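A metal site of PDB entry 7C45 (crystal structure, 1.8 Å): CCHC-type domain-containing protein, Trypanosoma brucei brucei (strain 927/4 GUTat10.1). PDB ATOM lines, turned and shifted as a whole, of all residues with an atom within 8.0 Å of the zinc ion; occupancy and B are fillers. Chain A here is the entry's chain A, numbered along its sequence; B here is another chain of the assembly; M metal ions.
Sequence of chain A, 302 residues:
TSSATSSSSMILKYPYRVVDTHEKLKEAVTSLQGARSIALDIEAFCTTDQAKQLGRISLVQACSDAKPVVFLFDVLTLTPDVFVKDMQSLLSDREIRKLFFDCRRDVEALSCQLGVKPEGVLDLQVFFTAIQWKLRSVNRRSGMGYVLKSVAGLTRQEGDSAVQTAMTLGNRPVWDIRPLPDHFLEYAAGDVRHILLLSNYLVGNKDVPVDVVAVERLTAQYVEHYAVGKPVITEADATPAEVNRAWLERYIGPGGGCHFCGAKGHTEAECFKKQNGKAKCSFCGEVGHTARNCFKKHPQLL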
ATOM      1  N   LYS A 280      -0.253   8.321 -27.081  1.00  0.00           N
ATOM      2  CA  LYS A 280      -0.862   9.625 -26.906  1.00  0.00           C
ATOM      3  C   LYS A 280      -2.362   9.537 -27.173  1.00  0.00           C
ATOM      4  O   LYS A 280      -2.832   8.679 -27.921  1.00  0.00           O
ATOM      5  CB  LYS A 280      -0.216  10.663 -27.844  1.00  0.00           C
ATOM      6  CG  LYS A 280       1.313  10.647 -27.868  1.00  0.00           C
ATOM      7  CD  LYS A 280       1.892  11.840 -28.607  1.00  0.00           C
ATOM      8  CE  LYS A 280       1.222  12.005 -29.953  1.00  0.00           C
ATOM      9  NZ  LYS A 280       1.289  10.749 -30.750  1.00  0.00           N
ATOM     10  N   CYS A 281      -3.108  10.457 -26.567  1.00  0.00           N
ATOM     11  CA  CYS A 281      -4.540  10.563 -26.854  1.00  0.00           C
ATOM     12  C   CYS A 281      -4.748  10.831 -28.340  1.00  0.00           C
ATOM     13  O   CYS A 281      -4.162  11.762 -28.891  1.00  0.00           O
ATOM     14  CB  CYS A 281      -5.170  11.680 -26.046  1.00  0.00           C
ATOM     15  SG  CYS A 281      -6.888  11.936 -26.471  1.00  0.00           S
ATOM     16  N   SER A 282      -5.554  10.003 -28.990  1.00  0.00           N
ATOM     17  CA  SER A 282      -5.744  10.170 -30.440  1.00  0.00           C
ATOM     18  C   SER A 282      -6.540  11.434 -30.787  1.00  0.00           C
ATOM     19  O   SER A 282      -6.520  11.881 -31.942  1.00  0.00           O
ATOM     20  CB  SER A 282      -6.413   8.944 -31.031  1.00  0.00           C
ATOM     21  OG  SER A 282      -7.704   8.768 -30.530  1.00  0.00           O
ATOM     22  N   PHE A 283      -7.229  12.018 -29.804  1.00  0.00           N
ATOM     23  CA  PHE A 283      -7.951  13.263 -30.041  1.00  0.00           C
ATOM     24  C   PHE A 283      -7.013  14.465 -29.895  1.00  0.00           C
ATOM     25  O   PHE A 283      -6.706  15.137 -30.871  1.00  0.00           O
ATOM     26  CB  PHE A 283      -9.152  13.372 -29.085  1.00  0.00           C
ATOM     27  CG  PHE A 283     -10.078  14.527 -29.406  1.00  0.00           C
ATOM     28  CD1 PHE A 283     -11.012  14.417 -30.403  1.00  0.00           C
ATOM     29  CD2 PHE A 283      -9.938  15.735 -28.756  1.00  0.00           C
ATOM     30  CE1 PHE A 283     -11.856  15.469 -30.697  1.00  0.00           C
ATOM     31  CE2 PHE A 283     -10.752  16.791 -29.050  1.00  0.00           C
ATOM     32  CZ  PHE A 283     -11.718  16.666 -30.034  1.00  0.00           C
ATOM     33  N   CYS A 284      -6.572  14.755 -28.670  1.00  0.00           N
ATOM     34  CA  CYS A 284      -5.814  15.971 -28.404  1.00  0.00           C
ATOM     35  C   CYS A 284      -4.312  15.803 -28.484  1.00  0.00           C
ATOM     36  O   CYS A 284      -3.573  16.799 -28.409  1.00  0.00           O
ATOM     37  CB  CYS A 284      -6.165  16.514 -27.014  1.00  0.00           C
ATOM     38  SG  CYS A 284      -5.489  15.474 -25.681  1.00  0.00           S
ATOM     39  N   GLY A 285      -3.829  14.567 -28.575  1.00  0.00           N
ATOM     40  CA  GLY A 285      -2.446  14.292 -28.836  1.00  0.00           C
ATOM     41  C   GLY A 285      -1.512  14.285 -27.641  1.00  0.00           C
ATOM     42  O   GLY A 285      -0.305  14.121 -27.826  1.00  0.00           O
ATOM     43  N   GLU A 286      -2.000  14.455 -26.416  1.00  0.00           N
ATOM     44  CA  GLU A 286      -1.073  14.469 -25.296  1.00  0.00           C
ATOM     45  C   GLU A 286      -0.959  13.090 -24.669  1.00  0.00           C
ATOM     46  O   GLU A 286      -1.827  12.225 -24.831  1.00  0.00           O
ATOM     47  CB  GLU A 286      -1.499  15.459 -24.224  1.00  0.00           C
ATOM     48  CG  GLU A 286      -2.435  16.405 -24.758  1.00  0.00           C
ATOM     49  CD  GLU A 286      -2.456  17.736 -24.073  1.00  0.00           C
ATOM     50  OE1 GLU A 286      -2.004  17.817 -22.919  1.00  0.00           O
ATOM     51  OE2 GLU A 286      -2.931  18.699 -24.702  1.00  0.00           O
ATOM     52  N   VAL A 287       0.137  12.900 -23.950  1.00  0.00           N
ATOM     53  CA  VAL A 287       0.398  11.654 -23.239  1.00  0.00           C
ATOM     54  C   VAL A 287      -0.383  11.682 -21.933  1.00  0.00           C
ATOM     55  O   VAL A 287      -0.640  12.737 -21.350  1.00  0.00           O
ATOM     56  CB  VAL A 287       1.916  11.484 -22.991  1.00  0.00           C
ATOM     57  CG1 VAL A 287       2.218  10.121 -22.410  1.00  0.00           C
ATOM     58  CG2 VAL A 287       2.689  11.693 -24.281  1.00  0.00           C
ATOM     59  N   GLY A 288      -0.808  10.503 -21.489  1.00  0.00           N
ATOM     60  CA  GLY A 288      -1.327  10.357 -20.148  1.00  0.00           C
ATOM     61  C   GLY A 288      -2.793  10.002 -20.065  1.00  0.00           C
ATOM     62  O   GLY A 288      -3.278   9.764 -18.957  1.00  0.00           O
ATOM     63  N   HIS A 289      -3.525   9.958 -21.194  1.00  0.00           N
ATOM     64  CA  HIS A 289      -4.910   9.524 -21.195  1.00  0.00           C
ATOM     65  C   HIS A 289      -5.299   9.037 -22.588  1.00  0.00           C
ATOM     66  O   HIS A 289      -4.601   9.296 -23.570  1.00  0.00           O
ATOM     67  CB  HIS A 289      -5.844  10.656 -20.735  1.00  0.00           C
ATOM     68  CG  HIS A 289      -5.938  11.795 -21.706  1.00  0.00           C
ATOM     69  ND1 HIS A 289      -5.151  12.913 -21.610  1.00  0.00           N
ATOM     70  CD2 HIS A 289      -6.711  11.963 -22.807  1.00  0.00           C
ATOM     71  CE1 HIS A 289      -5.421  13.732 -22.611  1.00  0.00           C
ATOM     72  NE2 HIS A 289      -6.376  13.182 -23.336  1.00  0.00           N
ATOM     73  N   THR A 290      -6.412   8.327 -22.660  1.00  0.00           N
ATOM     74  CA  THR A 290      -6.952   7.814 -23.917  1.00  0.00           C
ATOM     75  C   THR A 290      -8.062   8.725 -24.444  1.00  0.00           C
ATOM     76  O   THR A 290      -8.684   9.477 -23.698  1.00  0.00           O
ATOM     77  CB  THR A 290      -7.532   6.414 -23.748  1.00  0.00           C
ATOM     78  OG1 THR A 290      -8.683   6.518 -22.922  1.00  0.00           O
ATOM     79  CG2 THR A 290      -6.536   5.482 -23.107  1.00  0.00           C
ATOM     80  N   ALA A 291      -8.305   8.609 -25.758  1.00  0.00           N
ATOM     81  CA  ALA A 291      -9.412   9.316 -26.390  1.00  0.00           C
ATOM     82  C   ALA A 291     -10.734   9.080 -25.682  1.00  0.00           C
ATOM     83  O   ALA A 291     -11.539  10.007 -25.536  1.00  0.00           O
ATOM     84  CB  ALA A 291      -9.516   8.858 -27.850  1.00  0.00           C
ATOM     85  N   ARG A 292     -10.988   7.852 -25.227  1.00  0.00           N
ATOM     86  CA  ARG A 292     -12.256   7.538 -24.559  1.00  0.00           C
ATOM     87  C   ARG A 292     -12.447   8.359 -23.287  1.00  0.00           C
ATOM     88  O   ARG A 292     -13.590   8.605 -22.871  1.00  0.00           O
ATOM     89  CB  ARG A 292     -12.307   6.034 -24.223  1.00  0.00           C
ATOM     90  CG  ARG A 292     -13.705   5.493 -23.916  1.00  0.00           C
ATOM     91  CD  ARG A 292     -13.643   4.151 -23.163  1.00  0.00           C
ATOM     92  NE  ARG A 292     -14.974   3.627 -22.863  1.00  0.00           N
ATOM     93  CZ  ARG A 292     -15.761   4.088 -21.893  1.00  0.00           C
ATOM     94  NH1 ARG A 292     -15.340   5.087 -21.119  1.00  0.00           N
ATOM     95  NH2 ARG A 292     -16.974   3.561 -21.689  1.00  0.00           N
ATOM     96  N   ASN A 293     -11.353   8.811 -22.671  1.00  0.00           N
ATOM     97  CA  ASN A 293     -11.396   9.584 -21.423  1.00  0.00           C
ATOM     98  C   ASN A 293     -10.851  10.994 -21.611  1.00  0.00           C
ATOM     99  O   ASN A 293     -10.524  11.670 -20.641  1.00  0.00           O
ATOM    100  CB  ASN A 293     -10.639   8.853 -20.322  1.00  0.00           C
ATOM    101  CG  ASN A 293     -11.393   8.832 -19.002  1.00  0.00           C
ATOM    102  OD1 ASN A 293     -12.219   7.971 -18.771  1.00  0.00           O
ATOM    103  ND2 ASN A 293     -11.100   9.784 -18.124  1.00  0.00           N
ATOM    104  N   CYS A 294     -10.751  11.466 -22.858  1.00  0.00           N
ATOM    105  CA  CYS A 294     -10.227  12.796 -23.114  1.00  0.00           C
ATOM    106  C   CYS A 294     -11.243  13.859 -22.697  1.00  0.00           C
ATOM    107  O   CYS A 294     -12.388  13.851 -23.148  1.00  0.00           O
ATOM    108  CB  CYS A 294      -9.888  12.948 -24.607  1.00  0.00           C
ATOM    109  SG  CYS A 294      -9.325  14.584 -25.067  1.00  0.00           S
ATOM    110  N   PHE A 295     -10.802  14.793 -21.846  1.00  0.00           N
ATOM    111  CA  PHE A 295     -11.657  15.889 -21.392  1.00  0.00           C
ATOM    112  C   PHE A 295     -11.935  16.908 -22.496  1.00  0.00           C
ATOM    113  O   PHE A 295     -12.916  17.664 -22.404  1.00  0.00           O
ATOM    114  CB  PHE A 295     -11.013  16.571 -20.187  1.00  0.00           C
ATOM    115  CG  PHE A 295     -10.775  15.653 -19.005  1.00  0.00           C
ATOM    116  CD1 PHE A 295     -11.588  14.546 -18.799  1.00  0.00           C
ATOM    117  CD2 PHE A 295      -9.747  15.889 -18.108  1.00  0.00           C
ATOM    118  CE1 PHE A 295     -11.389  13.708 -17.699  1.00  0.00           C
ATOM    119  CE2 PHE A 295      -9.532  15.060 -17.022  1.00  0.00           C
ATOM    120  CZ  PHE A 295     -10.348  13.973 -16.806  1.00  0.00           C
ATOM    121  N   LYS A 296     -11.136  16.908 -23.556  1.00  0.00           N
ATOM    122  CA  LYS A 296     -11.377  17.829 -24.673  1.00  0.00           C
ATOM    123  C   LYS A 296     -12.460  17.255 -25.569  1.00  0.00           C
ATOM    124  O   LYS A 296     -13.342  17.948 -25.980  1.00  0.00           O
ATOM    125  CB  LYS A 296     -10.143  18.016 -25.499  1.00  0.00           C
ATOM    126  CG  LYS A 296      -8.940  18.468 -24.743  1.00  0.00           C
ATOM    127  CD  LYS A 296      -9.323  19.508 -23.730  1.00  0.00           C
ATOM    128  CE  LYS A 296      -8.360  20.635 -23.773  1.00  0.00           C
ATOM    129  NZ  LYS A 296      -7.472  20.873 -22.652  1.00  0.00           N
ATOM    130  N   LYS A 297     -12.328  15.986 -25.871  1.00  0.00           N
ATOM    131  CA  LYS A 297     -13.329  15.302 -26.683  1.00  0.00           C
ATOM    132  C   LYS A 297     -14.631  15.148 -25.922  1.00  0.00           C
ATOM    133  O   LYS A 297     -15.699  15.203 -26.524  1.00  0.00           O
ATOM    134  CB  LYS A 297     -12.804  13.933 -27.106  1.00  0.00           C
ATOM    135  CG  LYS A 297     -13.641  13.221 -28.147  1.00  0.00           C
ATOM    136  CD  LYS A 297     -12.908  11.971 -28.646  1.00  0.00           C
ATOM    137  CE  LYS A 297     -13.629  11.337 -29.858  1.00  0.00           C
ATOM    138  NZ  LYS A 297     -12.936  10.113 -30.409  1.00  0.00           N
ATOM    139  N   HIS A 298     -14.556  14.980 -24.605  1.00  0.00           N
ATOM    140  CA  HIS A 298     -15.713  14.672 -23.768  1.00  0.00           C
ATOM    141  C   HIS A 298     -15.700  15.580 -22.547  1.00  0.00           C
ATOM    142  O   HIS A 298     -15.356  15.154 -21.440  1.00  0.00           O
ATOM    143  CB  HIS A 298     -15.713  13.206 -23.321  1.00  0.00           C
ATOM    144  CG  HIS A 298     -15.467  12.227 -24.422  1.00  0.00           C
ATOM    145  ND1 HIS A 298     -16.468  11.794 -25.267  1.00  0.00           N
ATOM    146  CD2 HIS A 298     -14.352  11.558 -24.778  1.00  0.00           C
ATOM    147  CE1 HIS A 298     -15.971  10.916 -26.119  1.00  0.00           C
ATOM    148  NE2 HIS A 298     -14.692  10.742 -25.844  1.00  0.00           N
ATOM    149  O5'   U B   1      -2.030  18.412 -18.328  1.00  0.00           O
ATOM    150  C5'   U B   1      -1.877  18.703 -16.947  1.00  0.00           C
ATOM    151  C4'   U B   1      -3.120  18.379 -16.159  1.00  0.00           C
ATOM    152  O4'   U B   1      -4.198  19.262 -16.519  1.00  0.00           O
ATOM    153  C3'   U B   1      -3.723  16.983 -16.324  1.00  0.00           C
ATOM    154  O3'   U B   1      -3.054  16.042 -15.534  1.00  0.00           O
ATOM    155  C2'   U B   1      -5.178  17.179 -15.879  1.00  0.00           C
ATOM    156  O2'   U B   1      -5.276  17.027 -14.477  1.00  0.00           O
ATOM    157  C1'   U B   1      -5.437  18.655 -16.211  1.00  0.00           C
ATOM    158  N1    U B   1      -6.414  18.917 -17.302  1.00  0.00           N
ATOM    159  C2    U B   1      -6.370  18.286 -18.532  1.00  0.00           C
ATOM    160  O2    U B   1      -5.541  17.447 -18.852  1.00  0.00           O
ATOM    161  N3    U B   1      -7.350  18.686 -19.405  1.00  0.00           N
ATOM    162  C4    U B   1      -8.344  19.625 -19.189  1.00  0.00           C
ATOM    163  O4    U B   1      -9.168  19.878 -20.057  1.00  0.00           O
ATOM    164  C5    U B   1      -8.320  20.223 -17.894  1.00  0.00           C
ATOM    165  C6    U B   1      -7.391  19.855 -17.029  1.00  0.00           C
ATOM    166  P     U B   2      -2.457  14.680 -16.136  1.00  0.00           P
ATOM    167  OP1   U B   2      -1.305  14.348 -15.287  1.00  0.00           O
ATOM    168  OP2   U B   2      -2.292  14.794 -17.609  1.00  0.00           O
ATOM    169  O5'   U B   2      -3.592  13.612 -15.861  1.00  0.00           O
ATOM    170  C5'   U B   2      -4.124  13.413 -14.568  1.00  0.00           C
ATOM    171  C4'   U B   2      -5.097  12.255 -14.600  1.00  0.00           C
ATOM    172  O4'   U B   2      -6.266  12.662 -15.362  1.00  0.00           O
ATOM    173  C3'   U B   2      -4.541  10.993 -15.275  1.00  0.00           C
ATOM    174  O3'   U B   2      -5.050   9.848 -14.625  1.00  0.00           O
ATOM    175  C2'   U B   2      -5.133  11.068 -16.691  1.00  0.00           C
ATOM    176  O2'   U B   2      -5.324   9.814 -17.304  1.00  0.00           O
ATOM    177  C1'   U B   2      -6.472  11.768 -16.448  1.00  0.00           C
ATOM    178  N1    U B   2      -6.908  12.559 -17.598  1.00  0.00           N
ATOM    179  C2    U B   2      -7.985  12.072 -18.291  1.00  0.00           C
ATOM    180  O2    U B   2      -8.554  11.058 -17.936  1.00  0.00           O
ATOM    181  N3    U B   2      -8.363  12.813 -19.385  1.00  0.00           N
ATOM    182  C4    U B   2      -7.756  13.966 -19.851  1.00  0.00           C
ATOM    183  O4    U B   2      -8.213  14.547 -20.842  1.00  0.00           O
ATOM    184  C5    U B   2      -6.630  14.392 -19.082  1.00  0.00           C
ATOM    185  C6    U B   2      -6.244  13.693 -18.011  1.00  0.00           C
HETATM  186 ZN    ZN M   1      -7.079  13.923 -25.121  1.00  0.00          ZN
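O4 of U 2 of chain B sits close to a ring nitrogen (NE2) of His 289 (3.4 Å). SG of Cys 284 lies close to N of Glu 286 (3.7 Å). The side-chain sulfur (SG) of Cys 294 sits close to the backbone NH (N) of Lys 296 (3.3 Å). The side-chain sulfur of Cys 294 sits close to the backbone NH of Lys 297, 3.4 Å away. The side-chain sulfur of Cys 281 sits close to the backbone NH of Phe 283, at 3.4 Å. O of Glu 286 lies within hydrogen-bond range of N of Cys 281 (2.8 Å). SG of Cys 281 lies close to N of Ala 291 (3.7 Å).
The zinc ion is bound by NE2 of His 289 (2.1 Å), SG of Cys 284 (2.3 Å), SG of Cys 294 (2.3 Å) and SG of Cys 281 (2.4 Å).
The nearest printed residue that does not touch the zinc ion is U 2 of chain B (4.5 Å).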
